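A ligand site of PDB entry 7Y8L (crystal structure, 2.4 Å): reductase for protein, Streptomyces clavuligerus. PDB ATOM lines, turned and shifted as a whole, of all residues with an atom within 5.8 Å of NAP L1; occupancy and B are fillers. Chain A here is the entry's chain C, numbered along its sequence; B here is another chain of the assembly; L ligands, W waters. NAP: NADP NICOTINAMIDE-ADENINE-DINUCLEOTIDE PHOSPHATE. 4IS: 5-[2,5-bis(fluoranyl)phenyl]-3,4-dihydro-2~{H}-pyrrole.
The side-chain hydroxyl (OG) of Ser 94 is in hydrogen-bond range of the backbone NH (N) of Leu 68 (2.8 Å).
N of Leu 12 lies within hydrogen-bond range of OD1 of Asn 34 (3.3 Å).
NE of Arg 39 lies within hydrogen-bond range of O of Leu 12, at 3.3 Å.
OG of Ser 95 lies within hydrogen-bond range of ND1 of His 244 of chain B, at 3.1 Å.
The backbone carbonyl oxygen (O) of Thr 36 lies within hydrogen-bond range of the side-chain amide nitrogen (ND2) of Asn 34 (3.2 Å).
OD1 of Asp 70 sits at hydrogen-bond distance from N of Ala 73 (3.2 Å).
The backbone nitrogen (N) of Pro 14 sits close to an oxygen (O1N) of NAP L1 (3.5 Å).
Gly 11 touches NAP L1.
N of Gly 13 touches O3B of NAP L1, at 3.6 Å.
O of Ser 67 touches C4B of NAP L1, 3.3 Å away.
Ala 73 touches NAP L1 (CB to C5A, 3.6 Å).
Leu 77 touches NAP L1 (CD2 to C2A, 3.7 Å).
Leu 93 touches NAP L1.
CA of Ser 94 touches O3D of NAP L1 (3.6 Å).
O of Val 120 touches C5N of NAP L1 (3.4 Å).
Cys 122 touches NAP L1 (O to C4N, 3.3 Å).
CD of Pro 124 touches O7N of NAP L1, 3.5 Å away.
CB of Met 237 of chain B touches O1A of NAP L1, 3.2 Å away.
Hydrophobic or aromatic side chains within 4 Å of NAP L1: Pro 14, Met 15, Leu 68, Ala 73, Leu 77, Pro 124, Tyr 170 and Met 237 of chain B.
Of the 33 residues printed, 24 come within 4 Å of NAP L1.
Water W1 lies within hydrogen-bond range of the backbone carbonyl oxygen (O) of Ser 67 (2.8 Å), the backbone NH (N) of Gly 13 (2.9 Å), an oxygen (O1N) of NAP L1 (3.2 Å) and the backbone NH (N) of Gly 16 (3.2 Å).
O of Leu 68 sits at hydrogen-bond distance from O3D of NAP L1, 2.9 Å away.
O of Thr 69 is in hydrogen-bond range of O3D of NAP L1 (3.2 Å).
The guanidinium group of Arg 39 lies within salt-bridge range of an oxygen (O2X) of NAP L1, at 3.4 Å.
NE of Arg 35 lies within salt-bridge range of O1X of NAP L1 (2.8 Å).
The side-chain hydroxyl (OG1) of Thr 36 is in hydrogen-bond range of an oxygen (O1X) of NAP L1 (2.6 Å).
The backbone carbonyl oxygen (O) of Ala 232 of chain B sits at hydrogen-bond distance from a nitrogen (N7N) of NAP L1.
N of Thr 69 lies within hydrogen-bond range of O4B of NAP L1.
An oxygen (O3D) of NAP L1 lies within hydrogen-bond range of the backbone NH (N) of Ser 95.
N of Leu 12 sits at hydrogen-bond distance from O3B of NAP L1, 3.2 Å away.
An oxygen (O1X) of NAP L1 lies within hydrogen-bond range of the backbone NH (N) of Thr 36.
N of Met 15 lies within hydrogen-bond range of O1N of NAP L1 (2.7 Å).
An oxygen (O2D) of NAP L1 sits close to the side-chain hydroxyl of Tyr 170 (3.3 Å).
An oxygen (O1A) of NAP L1 sits at hydrogen-bond distance from the side-chain hydroxyl (OG1) of Thr 69 (2.6 Å).
The guanidinium group (NH1) of Arg 234 of chain B is in salt-bridge range of an oxygen (O2A) of NAP L1 (2.7 Å).
The side-chain amide nitrogen of Asn 34 is in hydrogen-bond range of an oxygen (O2X) of NAP L1 (2.8 Å).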
ATOM      1  N   GLY A  11     -20.231  15.312 -33.263  1.00  0.00           N
ATOM      2  CA  GLY A  11     -19.317  14.370 -32.618  1.00  0.00           C
ATOM      3  C   GLY A  11     -20.123  13.221 -32.054  1.00  0.00           C
ATOM      4  O   GLY A  11     -20.581  13.339 -30.902  1.00  0.00           O
ATOM      5  N   LEU A  12     -20.326  12.176 -32.841  1.00  0.00           N
ATOM      6  CA  LEU A  12     -21.205  11.076 -32.385  1.00  0.00           C
ATOM      7  C   LEU A  12     -20.377   9.798 -32.315  1.00  0.00           C
ATOM      8  O   LEU A  12     -20.727   8.828 -32.999  1.00  0.00           O
ATOM      9  CB  LEU A  12     -22.390  10.963 -33.352  1.00  0.00           C
ATOM     10  CG  LEU A  12     -23.665  11.702 -32.939  1.00  0.00           C
ATOM     11  CD1 LEU A  12     -23.438  13.203 -32.902  1.00  0.00           C
ATOM     12  CD2 LEU A  12     -24.804  11.365 -33.887  1.00  0.00           C
ATOM     13  N   GLY A  13     -19.301   9.827 -31.542  1.00  0.00           N
ATOM     14  CA  GLY A  13     -18.552   8.583 -31.274  1.00  0.00           C
ATOM     15  C   GLY A  13     -19.105   7.917 -30.028  1.00  0.00           C
ATOM     16  O   GLY A  13     -20.241   8.198 -29.672  1.00  0.00           O
ATOM     17  N   PRO A  14     -18.347   7.059 -29.316  1.00  0.00           N
ATOM     18  CA  PRO A  14     -18.835   6.481 -28.067  1.00  0.00           C
ATOM     19  C   PRO A  14     -19.396   7.515 -27.070  1.00  0.00           C
ATOM     20  O   PRO A  14     -20.444   7.258 -26.520  1.00  0.00           O
ATOM     21  CB  PRO A  14     -17.593   5.765 -27.537  1.00  0.00           C
ATOM     22  CG  PRO A  14     -16.841   5.363 -28.765  1.00  0.00           C
ATOM     23  CD  PRO A  14     -17.015   6.555 -29.684  1.00  0.00           C
ATOM     24  N   MET A  15     -18.732   8.653 -26.880  1.00  0.00           N
ATOM     25  CA  MET A  15     -19.142   9.671 -25.881  1.00  0.00           C
ATOM     26  C   MET A  15     -20.354  10.491 -26.358  1.00  0.00           C
ATOM     27  O   MET A  15     -21.341  10.511 -25.625  1.00  0.00           O
ATOM     28  CB  MET A  15     -18.008  10.653 -25.581  1.00  0.00           C
ATOM     29  CG  MET A  15     -16.914  10.063 -24.716  1.00  0.00           C
ATOM     30  SD  MET A  15     -17.514   9.594 -23.096  1.00  0.00           S
ATOM     31  CE  MET A  15     -17.381  11.157 -22.235  1.00  0.00           C
ATOM     32  N   GLY A  16     -20.258  11.149 -27.506  1.00  0.00           N
ATOM     33  CA  GLY A  16     -21.349  11.992 -28.015  1.00  0.00           C
ATOM     34  C   GLY A  16     -22.606  11.191 -28.289  1.00  0.00           C
ATOM     35  O   GLY A  16     -23.684  11.760 -28.151  1.00  0.00           O
ATOM     36  N   ASN A  34     -22.573  14.993 -38.064  1.00  0.00           N
ATOM     37  CA  ASN A  34     -21.327  14.202 -37.913  1.00  0.00           C
ATOM     38  C   ASN A  34     -20.648  14.010 -39.264  1.00  0.00           C
ATOM     39  O   ASN A  34     -21.367  13.879 -40.260  1.00  0.00           O
ATOM     40  CB  ASN A  34     -21.609  12.859 -37.231  1.00  0.00           C
ATOM     41  CG  ASN A  34     -20.421  12.299 -36.505  1.00  0.00           C
ATOM     42  OD1 ASN A  34     -19.611  13.047 -35.957  1.00  0.00           O
ATOM     43  ND2 ASN A  34     -20.295  10.982 -36.483  1.00  0.00           N
ATOM     44  N   ARG A  35     -19.307  14.051 -39.290  1.00  0.00           N
ATOM     45  CA  ARG A  35     -18.554  13.766 -40.526  1.00  0.00           C
ATOM     46  C   ARG A  35     -19.099  12.469 -41.102  1.00  0.00           C
ATOM     47  O   ARG A  35     -19.472  12.472 -42.277  1.00  0.00           O
ATOM     48  CB  ARG A  35     -17.062  13.615 -40.221  1.00  0.00           C
ATOM     49  CG  ARG A  35     -16.245  12.897 -41.285  1.00  0.00           C
ATOM     50  CD  ARG A  35     -14.786  12.827 -40.884  1.00  0.00           C
ATOM     51  NE  ARG A  35     -14.510  11.683 -40.026  1.00  0.00           N
ATOM     52  CZ  ARG A  35     -13.356  11.452 -39.426  1.00  0.00           C
ATOM     53  NH1 ARG A  35     -12.339  12.286 -39.583  1.00  0.00           N
ATOM     54  NH2 ARG A  35     -13.206  10.381 -38.668  1.00  0.00           N
ATOM     55  N   THR A  36     -19.127  11.413 -40.286  1.00  0.00           N
ATOM     56  CA  THR A  36     -19.769  10.168 -40.751  1.00  0.00           C
ATOM     57  C   THR A  36     -21.257  10.335 -40.436  1.00  0.00           C
ATOM     58  O   THR A  36     -21.613  10.220 -39.265  1.00  0.00           O
ATOM     59  CB  THR A  36     -19.135   8.930 -40.104  1.00  0.00           C
ATOM     60  OG1 THR A  36     -17.727   8.971 -40.338  1.00  0.00           O
ATOM     61  CG2 THR A  36     -19.701   7.642 -40.658  1.00  0.00           C
ATOM     62  N   ARG A  39     -23.472   7.758 -38.434  1.00  0.00           N
ATOM     63  CA  ARG A  39     -23.451   7.634 -36.957  1.00  0.00           C
ATOM     64  C   ARG A  39     -24.681   8.321 -36.376  1.00  0.00           C
ATOM     65  O   ARG A  39     -25.179   7.848 -35.328  1.00  0.00           O
ATOM     66  CB  ARG A  39     -22.156   8.184 -36.382  1.00  0.00           C
ATOM     67  CG  ARG A  39     -20.887   7.587 -36.992  1.00  0.00           C
ATOM     68  CD  ARG A  39     -20.271   6.472 -36.184  1.00  0.00           C
ATOM     69  NE  ARG A  39     -19.263   6.910 -35.230  1.00  0.00           N
ATOM     70  CZ  ARG A  39     -17.963   6.693 -35.330  1.00  0.00           C
ATOM     71  NH1 ARG A  39     -17.472   6.053 -36.380  1.00  0.00           N
ATOM     72  NH2 ARG A  39     -17.138   7.135 -34.400  1.00  0.00           N
ATOM     73  N   SER A  67     -17.950  16.555 -29.353  1.00  0.00           N
ATOM     74  CA  SER A  67     -17.216  15.370 -28.824  1.00  0.00           C
ATOM     75  C   SER A  67     -16.381  14.784 -29.962  1.00  0.00           C
ATOM     76  O   SER A  67     -16.820  13.828 -30.595  1.00  0.00           O
ATOM     77  CB  SER A  67     -18.128  14.358 -28.154  1.00  0.00           C
ATOM     78  OG  SER A  67     -17.377  13.449 -27.366  1.00  0.00           O
ATOM     79  N   LEU A  68     -15.208  15.369 -30.201  1.00  0.00           N
ATOM     80  CA  LEU A  68     -14.292  14.950 -31.292  1.00  0.00           C
ATOM     81  C   LEU A  68     -12.971  14.473 -30.696  1.00  0.00           C
ATOM     82  O   LEU A  68     -12.684  14.823 -29.551  1.00  0.00           O
ATOM     83  CB  LEU A  68     -14.098  16.179 -32.186  1.00  0.00           C
ATOM     84  CG  LEU A  68     -15.381  16.852 -32.649  1.00  0.00           C
ATOM     85  CD1 LEU A  68     -15.085  18.204 -33.288  1.00  0.00           C
ATOM     86  CD2 LEU A  68     -16.153  15.966 -33.602  1.00  0.00           C
ATOM     87  N   THR A  69     -12.164  13.725 -31.461  1.00  0.00           N
ATOM     88  CA  THR A  69     -10.883  13.178 -30.929  1.00  0.00           C
ATOM     89  C   THR A  69      -9.975  14.308 -30.452  1.00  0.00           C
ATOM     90  O   THR A  69      -9.249  14.101 -29.492  1.00  0.00           O
ATOM     91  CB  THR A  69     -10.166  12.297 -31.960  1.00  0.00           C
ATOM     92  OG1 THR A  69     -10.981  11.175 -32.257  1.00  0.00           O
ATOM     93  CG2 THR A  69      -8.810  11.807 -31.490  1.00  0.00           C
ATOM     94  N   ASP A  70     -10.038  15.464 -31.112  1.00  0.00           N
ATOM     95  CA  ASP A  70      -9.118  16.576 -30.764  1.00  0.00           C
ATOM     96  C   ASP A  70      -9.707  17.899 -31.235  1.00  0.00           C
ATOM     97  O   ASP A  70     -10.802  17.881 -31.811  1.00  0.00           O
ATOM     98  CB  ASP A  70      -7.731  16.331 -31.341  1.00  0.00           C
ATOM     99  CG  ASP A  70      -7.689  15.827 -32.775  1.00  0.00           C
ATOM    100  OD1 ASP A  70      -8.297  16.468 -33.643  1.00  0.00           O
ATOM    101  OD2 ASP A  70      -7.051  14.794 -33.007  1.00  0.00           O
ATOM    102  N   ASP A  72      -8.419  19.884 -33.550  1.00  0.00           N
ATOM    103  CA  ASP A  72      -8.242  20.000 -35.019  1.00  0.00           C
ATOM    104  C   ASP A  72      -9.530  19.562 -35.711  1.00  0.00           C
ATOM    105  O   ASP A  72      -9.895  20.186 -36.707  1.00  0.00           O
ATOM    106  CB  ASP A  72      -7.009  19.212 -35.481  1.00  0.00           C
ATOM    107  CG  ASP A  72      -6.872  19.104 -36.986  1.00  0.00           C
ATOM    108  OD1 ASP A  72      -6.342  20.055 -37.585  1.00  0.00           O
ATOM    109  OD2 ASP A  72      -7.280  18.076 -37.535  1.00  0.00           O
ATOM    110  N   ALA A  73     -10.176  18.504 -35.204  1.00  0.00           N
ATOM    111  CA  ALA A  73     -11.468  18.041 -35.753  1.00  0.00           C
ATOM    112  C   ALA A  73     -12.502  19.165 -35.718  1.00  0.00           C
ATOM    113  O   ALA A  73     -13.303  19.236 -36.646  1.00  0.00           O
ATOM    114  CB  ALA A  73     -11.927  16.840 -34.978  1.00  0.00           C
ATOM    115  N   ALA A  76     -11.982  21.484 -38.566  1.00  0.00           N
ATOM    116  CA  ALA A  76     -12.282  20.813 -39.836  1.00  0.00           C
ATOM    117  C   ALA A  76     -13.786  20.715 -40.053  1.00  0.00           C
ATOM    118  O   ALA A  76     -14.201  20.663 -41.203  1.00  0.00           O
ATOM    119  CB  ALA A  76     -11.631  19.461 -39.815  1.00  0.00           C
ATOM    120  N   LEU A  77     -14.564  20.700 -38.976  1.00  0.00           N
ATOM    121  CA  LEU A  77     -16.019  20.499 -39.110  1.00  0.00           C
ATOM    122  C   LEU A  77     -16.706  21.857 -39.123  1.00  0.00           C
ATOM    123  O   LEU A  77     -17.670  21.996 -39.869  1.00  0.00           O
ATOM    124  CB  LEU A  77     -16.484  19.626 -37.938  1.00  0.00           C
ATOM    125  CG  LEU A  77     -16.038  18.170 -38.018  1.00  0.00           C
ATOM    126  CD1 LEU A  77     -16.819  17.312 -37.040  1.00  0.00           C
ATOM    127  CD2 LEU A  77     -16.198  17.641 -39.435  1.00  0.00           C
ATOM    128  N   LEU A  93     -16.072  19.282 -25.623  1.00  0.00           N
ATOM    129  CA  LEU A  93     -15.730  18.233 -24.645  1.00  0.00           C
ATOM    130  C   LEU A  93     -14.686  17.326 -25.283  1.00  0.00           C
ATOM    131  O   LEU A  93     -14.756  16.113 -25.080  1.00  0.00           O
ATOM    132  CB  LEU A  93     -17.028  17.491 -24.317  1.00  0.00           C
ATOM    133  CG  LEU A  93     -18.134  18.375 -23.758  1.00  0.00           C
ATOM    134  CD1 LEU A  93     -19.390  17.565 -23.478  1.00  0.00           C
ATOM    135  CD2 LEU A  93     -17.666  19.040 -22.477  1.00  0.00           C
ATOM    136  N   SER A  94     -13.773  17.908 -26.027  1.00  0.00           N
ATOM    137  CA  SER A  94     -12.703  17.140 -26.703  1.00  0.00           C
ATOM    138  C   SER A  94     -11.367  17.357 -26.008  1.00  0.00           C
ATOM    139  O   SER A  94     -11.086  18.473 -25.574  1.00  0.00           O
ATOM    140  CB  SER A  94     -12.641  17.506 -28.149  1.00  0.00           C
ATOM    141  OG  SER A  94     -13.898  17.367 -28.765  1.00  0.00           O
ATOM    142  N   SER A  95     -10.578  16.292 -25.906  1.00  0.00           N
ATOM    143  CA  SER A  95      -9.243  16.375 -25.276  1.00  0.00           C
ATOM    144  C   SER A  95      -8.248  17.081 -26.192  1.00  0.00           C
ATOM    145  O   SER A  95      -8.315  16.871 -27.395  1.00  0.00           O
ATOM    146  CB  SER A  95      -8.723  15.016 -24.931  1.00  0.00           C
ATOM    147  OG  SER A  95      -7.514  15.101 -24.209  1.00  0.00           O
ATOM    148  N   VAL A 120     -14.613  15.630 -19.805  1.00  0.00           N
ATOM    149  CA  VAL A 120     -15.477  14.628 -19.129  1.00  0.00           C
ATOM    150  C   VAL A 120     -14.599  13.587 -18.427  1.00  0.00           C
ATOM    151  O   VAL A 120     -13.781  12.966 -19.092  1.00  0.00           O
ATOM    152  CB  VAL A 120     -16.468  14.001 -20.128  1.00  0.00           C
ATOM    153  CG1 VAL A 120     -17.734  13.539 -19.422  1.00  0.00           C
ATOM    154  CG2 VAL A 120     -16.827  14.962 -21.250  1.00  0.00           C
ATOM    155  N   THR A 121     -14.768  13.432 -17.124  1.00  0.00           N
ATOM    156  CA  THR A 121     -13.940  12.490 -16.325  1.00  0.00           C
ATOM    157  C   THR A 121     -14.670  11.154 -16.184  1.00  0.00           C
ATOM    158  O   THR A 121     -14.319  10.396 -15.283  1.00  0.00           O
ATOM    159  CB  THR A 121     -13.550  13.111 -14.981  1.00  0.00           C
ATOM    160  OG1 THR A 121     -14.696  13.174 -14.127  1.00  0.00           O
ATOM    161  CG2 THR A 121     -12.960  14.495 -15.126  1.00  0.00           C
ATOM    162  N   CYS A 122     -15.597  10.862 -17.088  1.00  0.00           N
ATOM    163  CA  CYS A 122     -16.399   9.616 -17.004  1.00  0.00           C
ATOM    164  C   CYS A 122     -16.350   8.859 -18.326  1.00  0.00           C
ATOM    165  O   CYS A 122     -16.070   9.464 -19.367  1.00  0.00           O
ATOM    166  CB  CYS A 122     -17.847   9.915 -16.667  1.00  0.00           C
ATOM    167  SG  CYS A 122     -18.841  10.638 -17.993  1.00  0.00           S
ATOM    168  N   PRO A 123     -16.635   7.532 -18.331  1.00  0.00           N
ATOM    169  CA  PRO A 123     -16.732   6.802 -19.572  1.00  0.00           C
ATOM    170  C   PRO A 123     -18.078   7.112 -20.244  1.00  0.00           C
ATOM    171  O   PRO A 123     -18.867   7.843 -19.706  1.00  0.00           O
ATOM    172  CB  PRO A 123     -16.675   5.352 -19.092  1.00  0.00           C
ATOM    173  CG  PRO A 123     -17.380   5.388 -17.775  1.00  0.00           C
ATOM    174  CD  PRO A 123     -16.852   6.664 -17.161  1.00  0.00           C
ATOM    175  N   PRO A 124     -18.367   6.583 -21.447  1.00  0.00           N
ATOM    176  CA  PRO A 124     -19.664   6.828 -22.072  1.00  0.00           C
ATOM    177  C   PRO A 124     -20.832   6.312 -21.209  1.00  0.00           C
ATOM    178  O   PRO A 124     -21.859   6.939 -21.212  1.00  0.00           O
ATOM    179  CB  PRO A 124     -19.530   6.115 -23.434  1.00  0.00           C
ATOM    180  CG  PRO A 124     -18.048   6.079 -23.691  1.00  0.00           C
ATOM    181  CD  PRO A 124     -17.473   5.804 -22.316  1.00  0.00           C
ATOM    182  N   TYR A 170      -7.937  17.704 -16.924  1.00  0.00           N
ATOM    183  CA  TYR A 170      -8.209  16.407 -17.560  1.00  0.00           C
ATOM    184  C   TYR A 170      -6.898  15.647 -17.754  1.00  0.00           C
ATOM    185  O   TYR A 170      -6.845  14.469 -17.453  1.00  0.00           O
ATOM    186  CB  TYR A 170      -8.948  16.650 -18.885  1.00  0.00           C
ATOM    187  CG  TYR A 170      -9.247  15.433 -19.714  1.00  0.00           C
ATOM    188  CD1 TYR A 170      -8.319  14.940 -20.612  1.00  0.00           C
ATOM    189  CD2 TYR A 170     -10.473  14.790 -19.632  1.00  0.00           C
ATOM    190  CE1 TYR A 170      -8.581  13.829 -21.381  1.00  0.00           C
ATOM    191  CE2 TYR A 170     -10.753  13.690 -20.413  1.00  0.00           C
ATOM    192  CZ  TYR A 170      -9.803  13.200 -21.291  1.00  0.00           C
ATOM    193  OH  TYR A 170     -10.052  12.107 -22.063  1.00  0.00           O
ATOM    194  N   ALA B 232     -16.664   1.343 -26.617  1.00  0.00           N
ATOM    195  CA  ALA B 232     -16.486   2.389 -25.594  1.00  0.00           C
ATOM    196  C   ALA B 232     -15.248   3.225 -25.903  1.00  0.00           C
ATOM    197  O   ALA B 232     -15.239   4.391 -25.493  1.00  0.00           O
ATOM    198  CB  ALA B 232     -16.395   1.759 -24.237  1.00  0.00           C
ATOM    199  N   ASP B 233     -14.239   2.651 -26.532  1.00  0.00           N
ATOM    200  CA  ASP B 233     -12.986   3.419 -26.740  1.00  0.00           C
ATOM    201  C   ASP B 233     -12.278   2.987 -28.005  1.00  0.00           C
ATOM    202  O   ASP B 233     -12.248   1.792 -28.273  1.00  0.00           O
ATOM    203  CB  ASP B 233     -12.053   3.314 -25.533  1.00  0.00           C
ATOM    204  CG  ASP B 233     -10.853   2.403 -25.683  1.00  0.00           C
ATOM    205  OD1 ASP B 233     -10.986   1.238 -25.331  1.00  0.00           O
ATOM    206  OD2 ASP B 233      -9.795   2.875 -26.148  1.00  0.00           O
ATOM    207  N   ARG B 234     -11.732   3.936 -28.742  1.00  0.00           N
ATOM    208  CA  ARG B 234     -10.914   3.567 -29.915  1.00  0.00           C
ATOM    209  C   ARG B 234      -9.462   3.877 -29.572  1.00  0.00           C
ATOM    210  O   ARG B 234      -9.193   4.955 -29.044  1.00  0.00           O
ATOM    211  CB  ARG B 234     -11.403   4.332 -31.143  1.00  0.00           C
ATOM    212  CG  ARG B 234     -12.758   3.905 -31.690  1.00  0.00           C
ATOM    213  CD  ARG B 234     -13.254   4.900 -32.712  1.00  0.00           C
ATOM    214  NE  ARG B 234     -12.325   5.125 -33.813  1.00  0.00           N
ATOM    215  CZ  ARG B 234     -11.655   6.256 -34.032  1.00  0.00           C
ATOM    216  NH1 ARG B 234     -11.792   7.289 -33.230  1.00  0.00           N
ATOM    217  NH2 ARG B 234     -10.829   6.337 -35.069  1.00  0.00           N
ATOM    218  N   MET B 237      -8.252   7.377 -30.610  1.00  0.00           N
ATOM    219  CA  MET B 237      -8.570   8.517 -29.718  1.00  0.00           C
ATOM    220  C   MET B 237      -7.689   8.470 -28.465  1.00  0.00           C
ATOM    221  O   MET B 237      -7.327   9.544 -27.992  1.00  0.00           O
ATOM    222  CB  MET B 237     -10.071   8.585 -29.372  1.00  0.00           C
ATOM    223  CG  MET B 237     -10.595   7.630 -28.359  1.00  0.00           C
ATOM    224  SD  MET B 237     -10.443   8.197 -26.672  1.00  0.00           S
ATOM    225  CE  MET B 237     -10.124   6.612 -25.902  1.00  0.00           C
ATOM    226  N   SER B 241      -5.161  11.145 -26.975  1.00  0.00           N
ATOM    227  CA  SER B 241      -5.265  11.504 -25.537  1.00  0.00           C
ATOM    228  C   SER B 241      -3.887  11.455 -24.856  1.00  0.00           C
ATOM    229  O   SER B 241      -3.590  12.388 -24.123  1.00  0.00           O
ATOM    230  CB  SER B 241      -6.231  10.581 -24.852  1.00  0.00           C
ATOM    231  OG  SER B 241      -6.193  10.727 -23.442  1.00  0.00           O
ATOM    232  N   HIS B 244      -1.794  14.113 -26.082  1.00  0.00           N
ATOM    233  CA  HIS B 244      -2.211  15.371 -25.446  1.00  0.00           C
ATOM    234  C   HIS B 244      -1.452  15.489 -24.132  1.00  0.00           C
ATOM    235  O   HIS B 244      -0.924  16.543 -23.883  1.00  0.00           O
ATOM    236  CB  HIS B 244      -3.735  15.440 -25.283  1.00  0.00           C
ATOM    237  CG  HIS B 244      -4.497  15.391 -26.562  1.00  0.00           C
ATOM    238  ND1 HIS B 244      -5.719  14.783 -26.668  1.00  0.00           N
ATOM    239  CD2 HIS B 244      -4.196  15.854 -27.794  1.00  0.00           C
ATOM    240  CE1 HIS B 244      -6.154  14.878 -27.911  1.00  0.00           C
ATOM    241  NE2 HIS B 244      -5.250  15.535 -28.614  1.00  0.00           N
HETATM  242  PA  NAP L   1     -13.659   9.332 -30.849  1.00  0.00           P
HETATM  243  O1A NAP L   1     -12.571  10.245 -30.426  1.00  0.00           O
HETATM  244  O2A NAP L   1     -13.368   7.889 -31.089  1.00  0.00           O
HETATM  245  O5B NAP L   1     -14.423   9.957 -32.096  1.00  0.00           O
HETATM  246  C5B NAP L   1     -15.255  11.084 -31.760  1.00  0.00           C
HETATM  247  C4B NAP L   1     -15.694  11.816 -32.992  1.00  0.00           C
HETATM  248  O4B NAP L   1     -14.569  12.520 -33.557  1.00  0.00           O
HETATM  249  C3B NAP L   1     -16.272  10.957 -34.132  1.00  0.00           C
HETATM  250  O3B NAP L   1     -17.626  11.350 -34.348  1.00  0.00           O
HETATM  251  C2B NAP L   1     -15.333  11.218 -35.311  1.00  0.00           C
HETATM  252  O2B NAP L   1     -16.058  11.391 -36.519  1.00  0.00           O
HETATM  253  C1B NAP L   1     -14.760  12.578 -34.941  1.00  0.00           C
HETATM  254  N9A NAP L   1     -13.477  12.900 -35.566  1.00  0.00           N
HETATM  255  C8A NAP L   1     -12.251  12.385 -35.263  1.00  0.00           C
HETATM  256  N7A NAP L   1     -11.277  12.885 -35.985  1.00  0.00           N
HETATM  257  C5A NAP L   1     -11.911  13.801 -36.813  1.00  0.00           C
HETATM  258  C6A NAP L   1     -11.426  14.659 -37.810  1.00  0.00           C
HETATM  259  N6A NAP L   1     -10.149  14.752 -38.164  1.00  0.00           N
HETATM  260  N1A NAP L   1     -12.326  15.437 -38.456  1.00  0.00           N
HETATM  261  C2A NAP L   1     -13.617  15.349 -38.103  1.00  0.00           C
HETATM  262  N3A NAP L   1     -14.184  14.586 -37.182  1.00  0.00           N
HETATM  263  C4A NAP L   1     -13.270  13.820 -36.568  1.00  0.00           C
HETATM  264  O3  NAP L   1     -14.795   9.417 -29.741  1.00  0.00           O
HETATM  265  PN  NAP L   1     -14.818   9.154 -28.176  1.00  0.00           P
HETATM  266  O1N NAP L   1     -16.228   9.333 -27.771  1.00  0.00           O
HETATM  267  O2N NAP L   1     -14.126   7.880 -27.870  1.00  0.00           O
HETATM  268  O5D NAP L   1     -13.948  10.365 -27.627  1.00  0.00           O
HETATM  269  C5D NAP L   1     -14.397  11.729 -27.812  1.00  0.00           C
HETATM  270  C4D NAP L   1     -13.544  12.656 -26.969  1.00  0.00           C
HETATM  271  O4D NAP L   1     -13.857  12.426 -25.571  1.00  0.00           O
HETATM  272  C3D NAP L   1     -12.026  12.505 -27.110  1.00  0.00           C
HETATM  273  O3D NAP L   1     -11.402  13.776 -27.198  1.00  0.00           O
HETATM  274  C2D NAP L   1     -11.642  11.722 -25.853  1.00  0.00           C
HETATM  275  O2D NAP L   1     -10.327  11.957 -25.392  1.00  0.00           O
HETATM  276  C1D NAP L   1     -12.681  12.198 -24.846  1.00  0.00           C
HETATM  277  N1N NAP L   1     -12.969  11.177 -23.797  1.00  0.00           N
HETATM  278  C2N NAP L   1     -13.017   9.843 -24.104  1.00  0.00           C
HETATM  279  C3N NAP L   1     -13.686   8.970 -23.291  1.00  0.00           C
HETATM  280  C7N NAP L   1     -13.995   7.597 -23.768  1.00  0.00           C
HETATM  281  O7N NAP L   1     -14.158   6.706 -22.939  1.00  0.00           O
HETATM  282  N7N NAP L   1     -14.114   7.366 -25.060  1.00  0.00           N
HETATM  283  C4N NAP L   1     -14.103   9.419 -21.959  1.00  0.00           C
HETATM  284  C5N NAP L   1     -13.873  10.847 -21.689  1.00  0.00           C
HETATM  285  C6N NAP L   1     -13.194  11.585 -22.519  1.00  0.00           C
HETATM  286  P2B NAP L   1     -16.509  10.030 -37.231  1.00  0.00           P
HETATM  287  O1X NAP L   1     -16.642  10.545 -38.626  1.00  0.00           O
HETATM  288  O2X NAP L   1     -17.836   9.579 -36.669  1.00  0.00           O
HETATM  289  O3X NAP L   1     -15.447   8.960 -37.112  1.00  0.00           O
HETATM  290  CAD 4IS L   2     -10.630   6.669 -22.074  1.00  0.00           C
HETATM  291  CAE 4IS L   2     -10.457   5.336 -22.742  1.00  0.00           C
HETATM  292  CAF 4IS L   2     -11.394   6.408 -20.953  1.00  0.00           C
HETATM  293  CAG 4IS L   2     -11.511   4.454 -22.104  1.00  0.00           C
HETATM  294  CAH 4IS L   2     -11.619   7.317 -20.002  1.00  0.00           C
HETATM  295  CAI 4IS L   2     -11.408   8.659 -20.249  1.00  0.00           C
HETATM  296  CAJ 4IS L   2     -12.058   6.916 -18.750  1.00  0.00           C
HETATM  297  CAK 4IS L   2     -12.300   7.871 -17.773  1.00  0.00           C
HETATM  298  CAL 4IS L   2     -11.653   9.606 -19.268  1.00  0.00           C
HETATM  299  CAM 4IS L   2     -12.096   9.212 -18.027  1.00  0.00           C
HETATM  300  FAA 4IS L   2     -11.010   9.051 -21.396  1.00  0.00           F
HETATM  301  FAB 4IS L   2     -12.677   7.532 -16.689  1.00  0.00           F
HETATM  302  NAC 4IS L   2     -11.926   5.197 -20.932  1.00  0.00           N
HETATM  303  O   HOH W   1     -17.832  11.437 -29.629  1.00  0.00           O
